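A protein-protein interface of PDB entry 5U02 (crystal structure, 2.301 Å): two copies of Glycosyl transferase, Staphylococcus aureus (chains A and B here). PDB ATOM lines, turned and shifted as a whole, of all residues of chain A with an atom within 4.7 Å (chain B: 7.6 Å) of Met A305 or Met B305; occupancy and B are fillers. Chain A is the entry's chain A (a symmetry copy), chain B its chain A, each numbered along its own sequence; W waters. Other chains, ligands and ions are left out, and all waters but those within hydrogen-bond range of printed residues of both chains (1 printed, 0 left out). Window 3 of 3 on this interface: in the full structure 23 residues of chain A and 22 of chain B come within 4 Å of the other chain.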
ATOM      1  N   GLU A 303      11.609   1.067  -5.748  1.00  0.00           N
ATOM      2  CA  GLU A 303      11.509   0.407  -7.037  1.00  0.00           C
ATOM      3  C   GLU A 303      11.608  -1.104  -6.868  1.00  0.00           C
ATOM      4  O   GLU A 303      12.206  -1.608  -5.914  1.00  0.00           O
ATOM      5  CB  GLU A 303      12.599   0.916  -7.985  1.00  0.00           C
ATOM      6  CG  GLU A 303      12.456   2.400  -8.329  1.00  0.00           C
ATOM      7  CD  GLU A 303      13.379   2.826  -9.454  1.00  0.00           C
ATOM      8  OE1 GLU A 303      14.585   2.517  -9.390  1.00  0.00           O
ATOM      9  OE2 GLU A 303      12.895   3.453 -10.417  1.00  0.00           O
ATOM     10  N   GLY A 304      11.002  -1.826  -7.803  1.00  0.00           N
ATOM     11  CA  GLY A 304      11.028  -3.273  -7.767  1.00  0.00           C
ATOM     12  C   GLY A 304       9.652  -3.881  -7.919  1.00  0.00           C
ATOM     13  O   GLY A 304       8.753  -3.261  -8.493  1.00  0.00           O
ATOM     14  N   MET A 305       9.475  -5.087  -7.387  1.00  0.00           N
ATOM     15  CA  MET A 305       8.221  -5.806  -7.556  1.00  0.00           C
ATOM     16  C   MET A 305       7.069  -5.062  -6.894  1.00  0.00           C
ATOM     17  O   MET A 305       7.227  -4.433  -5.843  1.00  0.00           O
ATOM     18  CB  MET A 305       8.337  -7.211  -6.975  1.00  0.00           C
ATOM     19  CG  MET A 305       9.397  -8.053  -7.655  1.00  0.00           C
ATOM     20  SD  MET A 305       9.728  -9.579  -6.763  1.00  0.00           S
ATOM     21  CE  MET A 305      11.206 -10.130  -7.611  1.00  0.00           C
ATOM     22  N   ALA A 306       5.903  -5.144  -7.525  1.00  0.00           N
ATOM     23  CA  ALA A 306       4.694  -4.518  -7.024  1.00  0.00           C
ATOM     24  C   ALA A 306       3.513  -5.327  -7.532  1.00  0.00           C
ATOM     25  O   ALA A 306       3.656  -6.186  -8.402  1.00  0.00           O
ATOM     26  CB  ALA A 306       4.602  -3.050  -7.458  1.00  0.00           C
ATOM     27  N   SER A 307       2.339  -5.053  -6.972  1.00  0.00           N
ATOM     28  CA  SER A 307       1.136  -5.748  -7.400  1.00  0.00           C
ATOM     29  C   SER A 307      -0.074  -4.866  -7.132  1.00  0.00           C
ATOM     30  O   SER A 307      -0.048  -4.001  -6.250  1.00  0.00           O
ATOM     31  CB  SER A 307       0.981  -7.099  -6.688  1.00  0.00           C
ATOM     32  OG  SER A 307       0.804  -6.929  -5.291  1.00  0.00           O
ATOM     33  N   MET A 316       0.652  -8.764 -10.902  1.00  0.00           N
ATOM     34  CA  MET A 316       1.992  -8.343 -10.529  1.00  0.00           C
ATOM     35  C   MET A 316       2.502  -7.291 -11.506  1.00  0.00           C
ATOM     36  O   MET A 316       1.999  -7.143 -12.623  1.00  0.00           O
ATOM     37  CB  MET A 316       2.957  -9.532 -10.516  1.00  0.00           C
ATOM     38  CG  MET A 316       2.674 -10.583  -9.447  1.00  0.00           C
ATOM     39  SD  MET A 316       2.989  -9.967  -7.782  1.00  0.00           S
ATOM     40  CE  MET A 316       4.715  -9.506  -7.909  1.00  0.00           C
ATOM     41  N   GLY A 317       3.522  -6.558 -11.073  1.00  0.00           N
ATOM     42  CA  GLY A 317       4.084  -5.508 -11.897  1.00  0.00           C
ATOM     43  C   GLY A 317       5.469  -5.138 -11.415  1.00  0.00           C
ATOM     44  O   GLY A 317       5.973  -5.674 -10.428  1.00  0.00           O
ATOM     45  N   MET A 318       6.088  -4.208 -12.139  1.00  0.00           N
ATOM     46  CA  MET A 318       7.394  -3.666 -11.781  1.00  0.00           C
ATOM     47  C   MET A 318       7.269  -2.159 -11.630  1.00  0.00           C
ATOM     48  O   MET A 318       6.820  -1.474 -12.557  1.00  0.00           O
ATOM     49  CB  MET A 318       8.447  -4.023 -12.829  1.00  0.00           C
ATOM     50  CG  MET A 318       9.247  -5.273 -12.484  1.00  0.00           C
ATOM     51  SD  MET A 318      10.515  -4.932 -11.245  1.00  0.00           S
ATOM     52  CE  MET A 318      11.397  -3.604 -12.059  1.00  0.00           C
ATOM     53  N   THR A 348       3.651  -2.224  -2.878  1.00  0.00           N
ATOM     54  CA  THR A 348       5.039  -2.154  -3.300  1.00  0.00           C
ATOM     55  C   THR A 348       5.767  -3.380  -2.753  1.00  0.00           C
ATOM     56  O   THR A 348       5.146  -4.311  -2.230  1.00  0.00           O
ATOM     57  CB  THR A 348       5.684  -0.848  -2.836  1.00  0.00           C
ATOM     58  OG1 THR A 348       5.706  -0.801  -1.405  1.00  0.00           O
ATOM     59  CG2 THR A 348       4.905   0.344  -3.369  1.00  0.00           C
ATOM     60  N   ALA A 349       7.100  -3.378  -2.845  1.00  0.00           N
ATOM     61  CA  ALA A 349       7.865  -4.565  -2.474  1.00  0.00           C
ATOM     62  C   ALA A 349       7.714  -4.918  -0.996  1.00  0.00           C
ATOM     63  O   ALA A 349       7.731  -6.102  -0.639  1.00  0.00           O
ATOM     64  CB  ALA A 349       9.340  -4.369  -2.824  1.00  0.00           C
ATOM     65  N   GLU B 302       2.800 -14.024   7.128  1.00  0.00           N
ATOM     66  CA  GLU B 302       2.984 -12.648   6.690  1.00  0.00           C
ATOM     67  C   GLU B 302       2.141 -12.378   5.449  1.00  0.00           C
ATOM     68  O   GLU B 302       2.155 -13.156   4.490  1.00  0.00           O
ATOM     69  CB  GLU B 302       4.458 -12.373   6.404  1.00  0.00           C
ATOM     70  CG  GLU B 302       5.154 -13.468   5.607  1.00  0.00           C
ATOM     71  CD  GLU B 302       6.488 -13.020   5.014  1.00  0.00           C
ATOM     72  OE1 GLU B 302       7.183 -13.871   4.421  1.00  0.00           O
ATOM     73  OE2 GLU B 302       6.835 -11.825   5.128  1.00  0.00           O
ATOM     74  N   GLU B 303       1.400 -11.279   5.469  1.00  0.00           N
ATOM     75  CA  GLU B 303       0.574 -10.932   4.326  1.00  0.00           C
ATOM     76  C   GLU B 303       1.421 -10.282   3.240  1.00  0.00           C
ATOM     77  O   GLU B 303       2.461  -9.678   3.508  1.00  0.00           O
ATOM     78  CB  GLU B 303      -0.566 -10.004   4.751  1.00  0.00           C
ATOM     79  CG  GLU B 303      -1.552 -10.659   5.720  1.00  0.00           C
ATOM     80  CD  GLU B 303      -2.799  -9.824   5.931  1.00  0.00           C
ATOM     81  OE1 GLU B 303      -2.672  -8.615   6.206  1.00  0.00           O
ATOM     82  OE2 GLU B 303      -3.912 -10.372   5.802  1.00  0.00           O
ATOM     83  N   GLY B 304       0.968 -10.423   1.999  1.00  0.00           N
ATOM     84  CA  GLY B 304       1.672  -9.845   0.873  1.00  0.00           C
ATOM     85  C   GLY B 304       1.904 -10.842  -0.239  1.00  0.00           C
ATOM     86  O   GLY B 304       1.164 -11.821  -0.368  1.00  0.00           O
ATOM     87  N   MET B 305       2.946 -10.613  -1.033  1.00  0.00           N
ATOM     88  CA  MET B 305       3.207 -11.454  -2.191  1.00  0.00           C
ATOM     89  C   MET B 305       3.516 -12.885  -1.771  1.00  0.00           C
ATOM     90  O   MET B 305       4.142 -13.132  -0.737  1.00  0.00           O
ATOM     91  CB  MET B 305       4.368 -10.887  -3.003  1.00  0.00           C
ATOM     92  CG  MET B 305       4.095  -9.499  -3.545  1.00  0.00           C
ATOM     93  SD  MET B 305       5.572  -8.733  -4.227  1.00  0.00           S
ATOM     94  CE  MET B 305       4.989  -7.053  -4.443  1.00  0.00           C
ATOM     95  N   ALA B 306       3.068 -13.826  -2.594  1.00  0.00           N
ATOM     96  CA  ALA B 306       3.293 -15.241  -2.363  1.00  0.00           C
ATOM     97  C   ALA B 306       3.292 -15.933  -3.715  1.00  0.00           C
ATOM     98  O   ALA B 306       2.916 -15.348  -4.731  1.00  0.00           O
ATOM     99  CB  ALA B 306       2.233 -15.831  -1.427  1.00  0.00           C
ATOM    100  N   SER B 307       3.731 -17.188  -3.725  1.00  0.00           N
ATOM    101  CA  SER B 307       3.750 -17.955  -4.960  1.00  0.00           C
ATOM    102  C   SER B 307       3.649 -19.436  -4.630  1.00  0.00           C
ATOM    103  O   SER B 307       4.024 -19.872  -3.537  1.00  0.00           O
ATOM    104  CB  SER B 307       5.017 -17.674  -5.780  1.00  0.00           C
ATOM    105  OG  SER B 307       6.181 -18.098  -5.091  1.00  0.00           O
ATOM    106  N   MET B 316       2.091 -16.736  -9.126  1.00  0.00           N
ATOM    107  CA  MET B 316       2.141 -15.729  -8.078  1.00  0.00           C
ATOM    108  C   MET B 316       0.759 -15.534  -7.470  1.00  0.00           C
ATOM    109  O   MET B 316      -0.265 -15.892  -8.058  1.00  0.00           O
ATOM    110  CB  MET B 316       2.648 -14.393  -8.626  1.00  0.00           C
ATOM    111  CG  MET B 316       4.098 -14.395  -9.099  1.00  0.00           C
ATOM    112  SD  MET B 316       5.263 -14.580  -7.736  1.00  0.00           S
ATOM    113  CE  MET B 316       4.832 -13.168  -6.722  1.00  0.00           C
ATOM    114  N   GLY B 317       0.738 -14.949  -6.277  1.00  0.00           N
ATOM    115  CA  GLY B 317      -0.512 -14.726  -5.581  1.00  0.00           C
ATOM    116  C   GLY B 317      -0.343 -13.675  -4.507  1.00  0.00           C
ATOM    117  O   GLY B 317       0.748 -13.148  -4.287  1.00  0.00           O
ATOM    118  N   MET B 318      -1.452 -13.369  -3.839  1.00  0.00           N
ATOM    119  CA  MET B 318      -1.468 -12.439  -2.715  1.00  0.00           C
ATOM    120  C   MET B 318      -2.029 -13.157  -1.499  1.00  0.00           C
ATOM    121  O   MET B 318      -3.139 -13.700  -1.551  1.00  0.00           O
ATOM    122  CB  MET B 318      -2.292 -11.193  -3.040  1.00  0.00           C
ATOM    123  CG  MET B 318      -1.455 -10.030  -3.555  1.00  0.00           C
ATOM    124  SD  MET B 318      -0.596  -9.181  -2.212  1.00  0.00           S
ATOM    125  CE  MET B 318      -1.987  -8.776  -1.161  1.00  0.00           C
ATOM    126  N   LEU B 319      -1.262 -13.163  -0.412  1.00  0.00           N
ATOM    127  CA  LEU B 319      -1.647 -13.857   0.808  1.00  0.00           C
ATOM    128  C   LEU B 319      -2.320 -12.880   1.757  1.00  0.00           C
ATOM    129  O   LEU B 319      -1.823 -11.771   1.971  1.00  0.00           O
ATOM    130  CB  LEU B 319      -0.430 -14.497   1.481  1.00  0.00           C
ATOM    131  CG  LEU B 319      -0.662 -15.439   2.670  1.00  0.00           C
ATOM    132  CD1 LEU B 319       0.454 -16.470   2.771  1.00  0.00           C
ATOM    133  CD2 LEU B 319      -0.785 -14.685   3.992  1.00  0.00           C
ATOM    134  N   ILE B 329      -4.694 -17.395  -0.377  1.00  0.00           N
ATOM    135  CA  ILE B 329      -3.699 -17.014  -1.367  1.00  0.00           C
ATOM    136  C   ILE B 329      -4.459 -16.800  -2.665  1.00  0.00           C
ATOM    137  O   ILE B 329      -4.885 -17.763  -3.311  1.00  0.00           O
ATOM    138  CB  ILE B 329      -2.596 -18.065  -1.517  1.00  0.00           C
ATOM    139  CG1 ILE B 329      -1.835 -18.220  -0.194  1.00  0.00           C
ATOM    140  CG2 ILE B 329      -1.640 -17.668  -2.636  1.00  0.00           C
ATOM    141  CD1 ILE B 329      -0.778 -19.303  -0.203  1.00  0.00           C
ATOM    142  N   ASN B 347       5.565 -20.500  -1.178  1.00  0.00           N
ATOM    143  CA  ASN B 347       6.402 -19.391  -0.739  1.00  0.00           C
ATOM    144  C   ASN B 347       5.546 -18.240  -0.236  1.00  0.00           C
ATOM    145  O   ASN B 347       4.539 -17.888  -0.854  1.00  0.00           O
ATOM    146  CB  ASN B 347       7.309 -18.890  -1.871  1.00  0.00           C
ATOM    147  CG  ASN B 347       8.503 -19.796  -2.108  1.00  0.00           C
ATOM    148  OD1 ASN B 347       8.363 -21.013  -2.213  1.00  0.00           O
ATOM    149  ND2 ASN B 347       9.689 -19.203  -2.187  1.00  0.00           N
ATOM    150  N   THR B 348       5.949 -17.663   0.894  1.00  0.00           N
ATOM    151  CA  THR B 348       5.460 -16.367   1.326  1.00  0.00           C
ATOM    152  C   THR B 348       6.470 -15.306   0.891  1.00  0.00           C
ATOM    153  O   THR B 348       7.402 -15.585   0.131  1.00  0.00           O
ATOM    154  CB  THR B 348       5.222 -16.350   2.836  1.00  0.00           C
ATOM    155  OG1 THR B 348       6.464 -16.549   3.523  1.00  0.00           O
ATOM    156  CG2 THR B 348       4.244 -17.444   3.229  1.00  0.00           C
ATOM    157  N   ALA B 349       6.306 -14.080   1.395  1.00  0.00           N
ATOM    158  CA  ALA B 349       7.139 -12.975   0.926  1.00  0.00           C
ATOM    159  C   ALA B 349       8.618 -13.184   1.246  1.00  0.00           C
ATOM    160  O   ALA B 349       9.483 -12.761   0.470  1.00  0.00           O
ATOM    161  CB  ALA B 349       6.649 -11.657   1.527  1.00  0.00           C
ATOM    162  N   HIS B 350       8.934 -13.834   2.365  1.00  0.00           N
ATOM    163  CA  HIS B 350      10.326 -14.018   2.759  1.00  0.00           C
ATOM    164  C   HIS B 350      10.724 -15.462   3.040  1.00  0.00           C
ATOM    165  O   HIS B 350      11.907 -15.708   3.302  1.00  0.00           O
ATOM    166  CB  HIS B 350      10.649 -13.190   4.012  1.00  0.00           C
ATOM    167  CG  HIS B 350      10.468 -11.714   3.835  1.00  0.00           C
ATOM    168  ND1 HIS B 350       9.273 -11.075   4.093  1.00  0.00           N
ATOM    169  CD2 HIS B 350      11.335 -10.747   3.453  1.00  0.00           C
ATOM    170  CE1 HIS B 350       9.409  -9.782   3.862  1.00  0.00           C
ATOM    171  NE2 HIS B 350      10.651  -9.557   3.471  1.00  0.00           N
ATOM    172  N   MET B 351       9.794 -16.414   3.016  1.00  0.00           N
ATOM    173  CA  MET B 351      10.092 -17.786   3.397  1.00  0.00           C
ATOM    174  C   MET B 351       9.609 -18.750   2.319  1.00  0.00           C
ATOM    175  O   MET B 351       8.702 -18.448   1.539  1.00  0.00           O
ATOM    176  CB  MET B 351       9.451 -18.139   4.747  1.00  0.00           C
ATOM    177  CG  MET B 351       9.535 -17.029   5.793  1.00  0.00           C
ATOM    178  SD  MET B 351      11.220 -16.623   6.310  1.00  0.00           S
ATOM    179  CE  MET B 351      11.688 -18.111   7.190  1.00  0.00           C
HETATM  180  O   HOH W   1       8.369  -8.225   1.474  1.00  0.00           O
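O of Ala A306 is in hydrogen-bond range of N of Gly A317, at 2.7 Å.
O of Met A305 is in hydrogen-bond range of N of Ala A349 (3.2 Å).
The backbone NH (N) of Ala B349 is in hydrogen-bond range of the backbone carbonyl oxygen (O) of Met B305, 3.2 Å away.
Met A305 touches Met B305.
Met B305 touches Ala A306.
Met B305 touches Met A316.
SD of Met A316 touches CE of Met B316, 3.8 Å away.
Thr A348 touches Met B305.
Of chain B, only Met B305 comes within 4 Å of Met A305.
Met B305 touches just these residues of chain A: Met A305, Ala A306, Met A316 and Thr A348.
Of the printed residues of chain B, Ala A306 touches Met B305.
Of the printed residues of chain B, Thr A348 touches Met B305.
Printed residues of chain B within 4 Å of Met A316: Met B305 and Met B316.
Printed residues of chain A within 4 Å of Met B316: Met A316.
Met B318 touches none of the printed residues of chain A.
The nearest residue of chain B that does not touch Met A305 is Met B316 (6.1 Å).
The nearest residue of chain A that does not touch Met B305 is Ser A307 (4.2 Å).
The nearest printed residue of chain B that does not touch Ala A306 is Met B316 (7.3 Å).
Hydrophobic or aromatic side chains of chain A that line the printed part of chain B: Met A316.
Printed residues of chain B that touch a printed residue of chain A: Met B305 and Met B316.
Among the printed residues, 5 pairs touch across the chains.
Met A305 touches its own counterpart, Met B305.
Ala A306 touches Met B305, but with the chains exchanged Met A305 does not touch Ala B306 (8.9 Å).
Met A316 touches Met B305, but with the chains exchanged Met A305 does not touch Met B316 (6.1 Å).
Thr A348 touches Met B305, but with the chains exchanged Met A305 does not touch Thr B348 (9.4 Å).
Positions printed for both chains: 303, 304, 305, 306, 307, 316, 317, 318, 348 and 349.
Of the 5 pairs that touch across the chains among the printed residues, 2 have their exchanged pair printed and touching as well.
Water W1 lies within hydrogen-bond range of the backbone carbonyl oxygen of Ala A349 (3.1 Å) and a ring nitrogen (NE2) of His B350 (3.3 Å).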
